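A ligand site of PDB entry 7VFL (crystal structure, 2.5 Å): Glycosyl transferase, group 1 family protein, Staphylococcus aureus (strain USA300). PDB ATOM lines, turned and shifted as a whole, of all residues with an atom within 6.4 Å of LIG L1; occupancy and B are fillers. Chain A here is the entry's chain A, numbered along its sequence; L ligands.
The backbone carbonyl oxygen (O) of Glu 407 sits at hydrogen-bond distance from the backbone NH (N) of Tyr 430, at 2.7 Å.
The side-chain carboxylate of Glu 407 sits at hydrogen-bond distance from the side-chain hydroxyl of Ser 404 (2.9 Å).
The backbone NH (N) of His 247 is in hydrogen-bond range of the side-chain hydroxyl (OH) of Tyr 266 (3.1 Å).
The side-chain hydroxyl (OH) of Tyr 266 is in hydrogen-bond range of the backbone NH (N) of Ser 248 (3.2 Å).
N of Val 305 lies within hydrogen-bond range of OG of Ser 282 (3.2 Å).
The side-chain sulfur (SD) of Met 406 is in hydrogen-bond range of the side-chain amino group (NZ) of Lys 263 (3.5 Å).
The backbone carbonyl oxygen (O) of Met 406 is in hydrogen-bond range of the side-chain hydroxyl (OG) of Ser 404, 3.0 Å away.
The side-chain carboxylate (OE2) of Glu 334 is in salt-bridge range of the guanidinium group (NH2) of Arg 330 (3.1 Å).
O2 of LIG L1 sits at hydrogen-bond distance from N of Gly 408 (2.8 Å).
The side-chain carboxylate of Glu 407 is in hydrogen-bond range of an oxygen (O2) of LIG L1 (2.9 Å).
A ring nitrogen (ND1) of His 247 is in hydrogen-bond range of an oxygen (O5) of LIG L1, at 3.0 Å.
An oxygen (O2) of LIG L1 is in hydrogen-bond range of the backbone NH (N) of Phe 409 (3.0 Å).
OG of Ser 248 lies within hydrogen-bond range of O1 of LIG L1 (3.0 Å).
An oxygen (O2) of LIG L1 sits at hydrogen-bond distance from the backbone NH (N) of Ser 410, 3.1 Å away.
N of Leu 411 is in hydrogen-bond range of O7 of LG2 L2, at 3.0 Å.
NE of Arg 330 lies within salt-bridge range of O12 of LG2 L2, at 2.8 Å.
NZ of Lys 335 lies within salt-bridge range of O10 of LG2 L2, 2.9 Å away.
N of Ala 412 is in hydrogen-bond range of O8 of LG2 L2 (3.0 Å).
An oxygen (O7) of LG2 L2 lies within hydrogen-bond range of an oxygen (O3) of LIG L1 (2.8 Å).
Merely in contact with LIG L1: Val 305, Met 406, Leu 411, Glu 334, Arg 330, Gly 16 and Ile 17.
Hydrophobic or aromatic side chains within 4 Å of LIG L1: Ile 17, His 247, Val 305, Phe 409 and Leu 411.
Within 4 Å of LIG L1: Gly 16, Ile 17, His 247, Ser 248, Val 305, Arg 330, Glu 334, Met 406, Glu 407, Gly 408, Phe 409, Ser 410 and Leu 411.
The nearest printed residue that does not touch LIG L1 is Ala 20 (4.2 Å).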
ATOM      1  N   GLY A  16      26.798 -24.421 -10.439  1.00  0.00           N
ATOM      2  CA  GLY A  16      25.372 -24.267 -10.647  1.00  0.00           C
ATOM      3  C   GLY A  16      24.609 -23.789  -9.442  1.00  0.00           C
ATOM      4  O   GLY A  16      23.980 -22.741  -9.483  1.00  0.00           O
ATOM      5  N   ILE A  17      24.653 -24.560  -8.366  1.00  0.00           N
ATOM      6  CA  ILE A  17      23.913 -24.240  -7.174  1.00  0.00           C
ATOM      7  C   ILE A  17      24.317 -22.881  -6.616  1.00  0.00           C
ATOM      8  O   ILE A  17      23.478 -22.104  -6.148  1.00  0.00           O
ATOM      9  CB  ILE A  17      24.097 -25.352  -6.142  1.00  0.00           C
ATOM     10  CG1 ILE A  17      23.460 -26.660  -6.632  1.00  0.00           C
ATOM     11  CG2 ILE A  17      23.487 -24.913  -4.816  1.00  0.00           C
ATOM     12  CD1 ILE A  17      23.228 -27.711  -5.496  1.00  0.00           C
ATOM     13  N   ALA A  20      22.828 -20.362  -8.831  1.00  0.00           N
ATOM     14  CA  ALA A  20      21.404 -20.204  -8.528  1.00  0.00           C
ATOM     15  C   ALA A  20      21.167 -19.303  -7.322  1.00  0.00           C
ATOM     16  O   ALA A  20      20.203 -18.524  -7.289  1.00  0.00           O
ATOM     17  CB  ALA A  20      20.772 -21.549  -8.257  1.00  0.00           C
ATOM     18  N   LEU A 246      15.141 -27.772  -4.314  1.00  0.00           N
ATOM     19  CA  LEU A 246      15.797 -28.847  -5.044  1.00  0.00           C
ATOM     20  C   LEU A 246      16.450 -28.262  -6.286  1.00  0.00           C
ATOM     21  O   LEU A 246      15.891 -27.390  -6.956  1.00  0.00           O
ATOM     22  CB  LEU A 246      14.818 -29.939  -5.448  1.00  0.00           C
ATOM     23  CG  LEU A 246      13.991 -30.490  -4.301  1.00  0.00           C
ATOM     24  CD1 LEU A 246      13.178 -31.691  -4.686  1.00  0.00           C
ATOM     25  CD2 LEU A 246      14.828 -30.919  -3.137  1.00  0.00           C
ATOM     26  N   HIS A 247      17.644 -28.749  -6.584  1.00  0.00           N
ATOM     27  CA  HIS A 247      18.421 -28.278  -7.716  1.00  0.00           C
ATOM     28  C   HIS A 247      18.724 -29.357  -8.745  1.00  0.00           C
ATOM     29  O   HIS A 247      19.240 -29.032  -9.814  1.00  0.00           O
ATOM     30  CB  HIS A 247      19.749 -27.700  -7.226  1.00  0.00           C
ATOM     31  CG  HIS A 247      19.608 -26.408  -6.486  1.00  0.00           C
ATOM     32  ND1 HIS A 247      19.610 -25.184  -7.111  1.00  0.00           N
ATOM     33  CD2 HIS A 247      19.448 -26.156  -5.164  1.00  0.00           C
ATOM     34  CE1 HIS A 247      19.475 -24.230  -6.214  1.00  0.00           C
ATOM     35  NE2 HIS A 247      19.359 -24.792  -5.024  1.00  0.00           N
ATOM     36  N   SER A 248      18.418 -30.616  -8.459  1.00  0.00           N
ATOM     37  CA  SER A 248      18.631 -31.729  -9.374  1.00  0.00           C
ATOM     38  C   SER A 248      17.371 -32.591  -9.414  1.00  0.00           C
ATOM     39  O   SER A 248      16.415 -32.395  -8.663  1.00  0.00           O
ATOM     40  CB  SER A 248      19.785 -32.606  -8.910  1.00  0.00           C
ATOM     41  OG  SER A 248      20.939 -31.820  -8.874  1.00  0.00           O
ATOM     42  N   THR A 249      17.382 -33.597 -10.274  1.00  0.00           N
ATOM     43  CA  THR A 249      16.504 -34.743 -10.035  1.00  0.00           C
ATOM     44  C   THR A 249      16.581 -35.160  -8.559  1.00  0.00           C
ATOM     45  O   THR A 249      17.639 -35.093  -7.921  1.00  0.00           O
ATOM     46  CB  THR A 249      16.864 -35.919 -10.920  1.00  0.00           C
ATOM     47  OG1 THR A 249      18.265 -36.163 -10.765  1.00  0.00           O
ATOM     48  CG2 THR A 249      16.541 -35.612 -12.356  1.00  0.00           C
ATOM     49  N   LYS A 263      17.652 -39.430  -3.740  1.00  0.00           N
ATOM     50  CA  LYS A 263      19.085 -39.204  -3.678  1.00  0.00           C
ATOM     51  C   LYS A 263      19.515 -38.977  -2.238  1.00  0.00           C
ATOM     52  O   LYS A 263      18.766 -38.475  -1.386  1.00  0.00           O
ATOM     53  CB  LYS A 263      19.485 -37.992  -4.523  1.00  0.00           C
ATOM     54  CG  LYS A 263      19.491 -38.272  -6.006  1.00  0.00           C
ATOM     55  CD  LYS A 263      20.163 -37.180  -6.767  1.00  0.00           C
ATOM     56  CE  LYS A 263      19.852 -37.258  -8.200  1.00  0.00           C
ATOM     57  NZ  LYS A 263      20.355 -36.028  -8.860  1.00  0.00           N
ATOM     58  N   TYR A 266      19.054 -35.531  -0.591  1.00  0.00           N
ATOM     59  CA  TYR A 266      17.705 -35.083  -0.232  1.00  0.00           C
ATOM     60  C   TYR A 266      17.023 -35.956   0.790  1.00  0.00           C
ATOM     61  O   TYR A 266      15.990 -35.538   1.324  1.00  0.00           O
ATOM     62  CB  TYR A 266      16.784 -34.963  -1.479  1.00  0.00           C
ATOM     63  CG  TYR A 266      17.312 -34.014  -2.574  1.00  0.00           C
ATOM     64  CD1 TYR A 266      17.717 -32.745  -2.261  1.00  0.00           C
ATOM     65  CD2 TYR A 266      17.392 -34.381  -3.874  1.00  0.00           C
ATOM     66  CE1 TYR A 266      18.233 -31.883  -3.202  1.00  0.00           C
ATOM     67  CE2 TYR A 266      17.916 -33.505  -4.842  1.00  0.00           C
ATOM     68  CZ  TYR A 266      18.345 -32.248  -4.471  1.00  0.00           C
ATOM     69  OH  TYR A 266      18.843 -31.334  -5.346  1.00  0.00           O
ATOM     70  N   SER A 282      12.748 -26.226 -10.337  1.00  0.00           N
ATOM     71  CA  SER A 282      12.897 -25.282 -11.441  1.00  0.00           C
ATOM     72  C   SER A 282      11.872 -25.473 -12.564  1.00  0.00           C
ATOM     73  O   SER A 282      11.557 -24.519 -13.290  1.00  0.00           O
ATOM     74  CB  SER A 282      14.293 -25.376 -12.053  1.00  0.00           C
ATOM     75  OG  SER A 282      15.275 -24.758 -11.225  1.00  0.00           O
ATOM     76  N   VAL A 305      15.649 -21.567 -11.675  1.00  0.00           N
ATOM     77  CA  VAL A 305      16.820 -20.999 -11.004  1.00  0.00           C
ATOM     78  C   VAL A 305      17.592 -19.994 -11.872  1.00  0.00           C
ATOM     79  O   VAL A 305      18.489 -19.330 -11.363  1.00  0.00           O
ATOM     80  CB  VAL A 305      17.860 -22.051 -10.582  1.00  0.00           C
ATOM     81  CG1 VAL A 305      17.353 -22.896  -9.370  1.00  0.00           C
ATOM     82  CG2 VAL A 305      18.129 -23.002 -11.742  1.00  0.00           C
ATOM     83  N   ARG A 330      30.421 -29.161 -16.840  1.00  0.00           N
ATOM     84  CA  ARG A 330      31.453 -29.801 -16.044  1.00  0.00           C
ATOM     85  C   ARG A 330      32.005 -31.046 -16.758  1.00  0.00           C
ATOM     86  O   ARG A 330      31.297 -31.732 -17.493  1.00  0.00           O
ATOM     87  CB  ARG A 330      30.891 -30.192 -14.670  1.00  0.00           C
ATOM     88  CG  ARG A 330      30.850 -29.021 -13.658  1.00  0.00           C
ATOM     89  CD  ARG A 330      30.097 -29.408 -12.411  1.00  0.00           C
ATOM     90  NE  ARG A 330      28.741 -29.852 -12.743  1.00  0.00           N
ATOM     91  CZ  ARG A 330      28.301 -31.097 -12.596  1.00  0.00           C
ATOM     92  NH1 ARG A 330      29.098 -32.063 -12.179  1.00  0.00           N
ATOM     93  NH2 ARG A 330      27.027 -31.363 -12.855  1.00  0.00           N
ATOM     94  N   GLU A 334      27.916 -37.624 -15.775  1.00  0.00           N
ATOM     95  CA  GLU A 334      26.528 -37.464 -16.214  1.00  0.00           C
ATOM     96  C   GLU A 334      26.347 -36.490 -17.393  1.00  0.00           C
ATOM     97  O   GLU A 334      25.272 -36.473 -17.982  1.00  0.00           O
ATOM     98  CB  GLU A 334      25.688 -36.963 -15.042  1.00  0.00           C
ATOM     99  CG  GLU A 334      25.936 -35.477 -14.687  1.00  0.00           C
ATOM    100  CD  GLU A 334      26.823 -35.295 -13.474  1.00  0.00           C
ATOM    101  OE1 GLU A 334      27.860 -36.014 -13.368  1.00  0.00           O
ATOM    102  OE2 GLU A 334      26.466 -34.441 -12.612  1.00  0.00           O
ATOM    103  N   LYS A 335      27.313 -35.622 -17.673  1.00  0.00           N
ATOM    104  CA  LYS A 335      27.241 -34.821 -18.892  1.00  0.00           C
ATOM    105  C   LYS A 335      27.611 -35.617 -20.146  1.00  0.00           C
ATOM    106  O   LYS A 335      27.308 -35.174 -21.258  1.00  0.00           O
ATOM    107  CB  LYS A 335      28.175 -33.609 -18.763  1.00  0.00           C
ATOM    108  CG  LYS A 335      28.004 -32.774 -17.512  1.00  0.00           C
ATOM    109  CD  LYS A 335      26.591 -32.172 -17.387  1.00  0.00           C
ATOM    110  CE  LYS A 335      26.601 -30.970 -16.408  1.00  0.00           C
ATOM    111  NZ  LYS A 335      25.231 -30.430 -16.203  1.00  0.00           N
ATOM    112  N   SER A 404      23.677 -34.589 -21.640  1.00  0.00           N
ATOM    113  CA  SER A 404      23.560 -34.986 -20.257  1.00  0.00           C
ATOM    114  C   SER A 404      22.428 -35.978 -20.102  1.00  0.00           C
ATOM    115  O   SER A 404      21.485 -35.993 -20.907  1.00  0.00           O
ATOM    116  CB  SER A 404      23.290 -33.743 -19.407  1.00  0.00           C
ATOM    117  OG  SER A 404      23.053 -34.012 -18.056  1.00  0.00           O
ATOM    118  N   MET A 406      20.905 -36.101 -16.980  1.00  0.00           N
ATOM    119  CA  MET A 406      20.347 -35.701 -15.695  1.00  0.00           C
ATOM    120  C   MET A 406      20.595 -34.222 -15.491  1.00  0.00           C
ATOM    121  O   MET A 406      21.752 -33.798 -15.376  1.00  0.00           O
ATOM    122  CB  MET A 406      21.001 -36.518 -14.582  1.00  0.00           C
ATOM    123  CG  MET A 406      20.571 -36.195 -13.149  1.00  0.00           C
ATOM    124  SD  MET A 406      21.685 -36.934 -11.915  1.00  0.00           S
ATOM    125  CE  MET A 406      23.294 -36.573 -12.615  1.00  0.00           C
ATOM    126  N   GLU A 407      19.510 -33.455 -15.415  1.00  0.00           N
ATOM    127  CA  GLU A 407      19.614 -32.050 -15.077  1.00  0.00           C
ATOM    128  C   GLU A 407      18.488 -31.653 -14.120  1.00  0.00           C
ATOM    129  O   GLU A 407      17.445 -32.313 -14.028  1.00  0.00           O
ATOM    130  CB  GLU A 407      19.558 -31.161 -16.343  1.00  0.00           C
ATOM    131  CG  GLU A 407      20.706 -31.337 -17.346  1.00  0.00           C
ATOM    132  CD  GLU A 407      22.035 -30.736 -16.895  1.00  0.00           C
ATOM    133  OE1 GLU A 407      22.075 -29.866 -16.015  1.00  0.00           O
ATOM    134  OE2 GLU A 407      23.074 -31.197 -17.400  1.00  0.00           O
ATOM    135  N   GLY A 408      18.709 -30.559 -13.405  1.00  0.00           N
ATOM    136  CA  GLY A 408      17.616 -29.900 -12.719  1.00  0.00           C
ATOM    137  C   GLY A 408      16.930 -28.811 -13.528  1.00  0.00           C
ATOM    138  O   GLY A 408      15.715 -28.594 -13.413  1.00  0.00           O
ATOM    139  N   PHE A 409      17.726 -28.121 -14.358  1.00  0.00           N
ATOM    140  CA  PHE A 409      17.236 -27.030 -15.208  1.00  0.00           C
ATOM    141  C   PHE A 409      18.174 -26.865 -16.393  1.00  0.00           C
ATOM    142  O   PHE A 409      17.727 -26.876 -17.553  1.00  0.00           O
ATOM    143  CB  PHE A 409      17.137 -25.729 -14.378  1.00  0.00           C
ATOM    144  CG  PHE A 409      16.742 -24.549 -15.163  1.00  0.00           C
ATOM    145  CD1 PHE A 409      15.464 -24.402 -15.610  1.00  0.00           C
ATOM    146  CD2 PHE A 409      17.621 -23.544 -15.421  1.00  0.00           C
ATOM    147  CE1 PHE A 409      15.074 -23.288 -16.328  1.00  0.00           C
ATOM    148  CE2 PHE A 409      17.223 -22.440 -16.143  1.00  0.00           C
ATOM    149  CZ  PHE A 409      15.932 -22.353 -16.624  1.00  0.00           C
ATOM    150  N   SER A 410      19.473 -26.712 -16.077  1.00  0.00           N
ATOM    151  CA  SER A 410      20.591 -26.387 -16.946  1.00  0.00           C
ATOM    152  C   SER A 410      20.684 -24.882 -17.162  1.00  0.00           C
ATOM    153  O   SER A 410      20.141 -24.336 -18.138  1.00  0.00           O
ATOM    154  CB  SER A 410      20.513 -27.109 -18.286  1.00  0.00           C
ATOM    155  OG  SER A 410      21.643 -26.699 -19.064  1.00  0.00           O
ATOM    156  N   LEU A 411      21.469 -24.226 -16.299  1.00  0.00           N
ATOM    157  CA  LEU A 411      21.716 -22.794 -16.473  1.00  0.00           C
ATOM    158  C   LEU A 411      22.431 -22.539 -17.784  1.00  0.00           C
ATOM    159  O   LEU A 411      22.212 -21.527 -18.438  1.00  0.00           O
ATOM    160  CB  LEU A 411      22.534 -22.221 -15.313  1.00  0.00           C
ATOM    161  CG  LEU A 411      21.880 -22.290 -13.935  1.00  0.00           C
ATOM    162  CD1 LEU A 411      22.882 -22.181 -12.842  1.00  0.00           C
ATOM    163  CD2 LEU A 411      20.902 -21.168 -13.795  1.00  0.00           C
ATOM    164  N   ALA A 412      23.336 -23.427 -18.160  1.00  0.00           N
ATOM    165  CA  ALA A 412      24.044 -23.258 -19.421  1.00  0.00           C
ATOM    166  C   ALA A 412      23.124 -23.302 -20.648  1.00  0.00           C
ATOM    167  O   ALA A 412      23.393 -22.624 -21.643  1.00  0.00           O
ATOM    168  CB  ALA A 412      25.106 -24.334 -19.484  1.00  0.00           C
ATOM    169  N   TYR A 430      15.750 -32.908 -16.025  1.00  0.00           N
ATOM    170  CA  TYR A 430      14.630 -31.960 -16.212  1.00  0.00           C
ATOM    171  C   TYR A 430      15.139 -30.663 -16.818  1.00  0.00           C
ATOM    172  O   TYR A 430      16.245 -30.238 -16.465  1.00  0.00           O
ATOM    173  CB  TYR A 430      13.992 -31.566 -14.881  1.00  0.00           C
ATOM    174  CG  TYR A 430      13.220 -32.648 -14.173  1.00  0.00           C
ATOM    175  CD1 TYR A 430      11.941 -32.982 -14.581  1.00  0.00           C
ATOM    176  CD2 TYR A 430      13.763 -33.315 -13.097  1.00  0.00           C
ATOM    177  CE1 TYR A 430      11.231 -33.978 -13.925  1.00  0.00           C
ATOM    178  CE2 TYR A 430      13.077 -34.318 -12.445  1.00  0.00           C
ATOM    179  CZ  TYR A 430      11.800 -34.641 -12.862  1.00  0.00           C
ATOM    180  OH  TYR A 430      11.113 -35.623 -12.217  1.00  0.00           O
HETATM  181  C1  LIG L   1      22.535 -28.601 -10.667  1.00  0.00           C
HETATM  182  C2  LIG L   1      21.774 -29.171 -11.872  1.00  0.00           C
HETATM  183  C3  LIG L   1      21.494 -28.056 -12.872  1.00  0.00           C
HETATM  184  C4  LIG L   1      20.844 -26.863 -12.198  1.00  0.00           C
HETATM  185  C5  LIG L   1      21.687 -26.421 -11.005  1.00  0.00           C
HETATM  186  C6  LIG L   1      21.053 -25.228 -10.316  1.00  0.00           C
HETATM  187  C7  LIG L   1      22.354 -31.500 -12.334  1.00  0.00           C
HETATM  188  C8  LIG L   1      23.489 -32.380 -12.761  1.00  0.00           C
HETATM  189  N1  LIG L   1      22.532 -30.207 -12.541  1.00  0.00           N
HETATM  190  O1  LIG L   1      22.737 -29.596  -9.665  1.00  0.00           O
HETATM  191  O2  LIG L   1      20.614 -28.550 -13.882  1.00  0.00           O
HETATM  192  O3  LIG L   1      20.770 -25.794 -13.136  1.00  0.00           O
HETATM  193  O4  LIG L   1      21.796 -27.513 -10.101  1.00  0.00           O
HETATM  194  O5  LIG L   1      19.682 -25.515 -10.046  1.00  0.00           O
HETATM  195  O6  LIG L   1      21.344 -31.957 -11.852  1.00  0.00           O
HETATM  196  N1  LG2 L   2      30.273 -22.117 -16.307  1.00  0.00           N
HETATM  197  C1  LG2 L   2      31.161 -21.030 -16.434  1.00  0.00           C
HETATM  198  N2  LG2 L   2      32.283 -21.167 -17.132  1.00  0.00           N
HETATM  199  C2  LG2 L   2      32.596 -22.316 -17.710  1.00  0.00           C
HETATM  200  C3  LG2 L   2      31.746 -23.395 -17.601  1.00  0.00           C
HETATM  201  C4  LG2 L   2      30.565 -23.279 -16.883  1.00  0.00           C
HETATM  202  O1  LG2 L   2      30.899 -19.941 -15.890  1.00  0.00           O
HETATM  203  O2  LG2 L   2      33.650 -22.407 -18.350  1.00  0.00           O
HETATM  204  C5  LG2 L   2      29.045 -21.942 -15.532  1.00  0.00           C
HETATM  205  C6  LG2 L   2      27.860 -21.798 -16.459  1.00  0.00           C
HETATM  206  O3  LG2 L   2      27.697 -20.431 -16.811  1.00  0.00           O
HETATM  207  C7  LG2 L   2      26.705 -22.346 -15.655  1.00  0.00           C
HETATM  208  C8  LG2 L   2      27.329 -23.214 -14.591  1.00  0.00           C
HETATM  209  O4  LG2 L   2      28.746 -23.074 -14.727  1.00  0.00           O
HETATM  210  O5  LG2 L   2      25.957 -21.304 -15.045  1.00  0.00           O
HETATM  211  C9  LG2 L   2      26.936 -24.667 -14.755  1.00  0.00           C
HETATM  212  O6  LG2 L   2      25.593 -24.836 -14.300  1.00  0.00           O
HETATM  213  P1  LG2 L   2      24.564 -25.815 -15.024  1.00  0.00           P
HETATM  214  O7  LG2 L   2      23.236 -25.715 -14.367  1.00  0.00           O
HETATM  215  O8  LG2 L   2      24.654 -25.576 -16.492  1.00  0.00           O
HETATM  216  O9  LG2 L   2      25.171 -27.261 -14.759  1.00  0.00           O
HETATM  217  P2  LG2 L   2      25.468 -27.896 -13.324  1.00  0.00           P
HETATM  218  O10 LG2 L   2      24.990 -29.290 -13.508  1.00  0.00           O
HETATM  219  O11 LG2 L   2      24.718 -27.093 -12.324  1.00  0.00           O
HETATM  220  O12 LG2 L   2      26.942 -27.736 -13.141  1.00  0.00           O
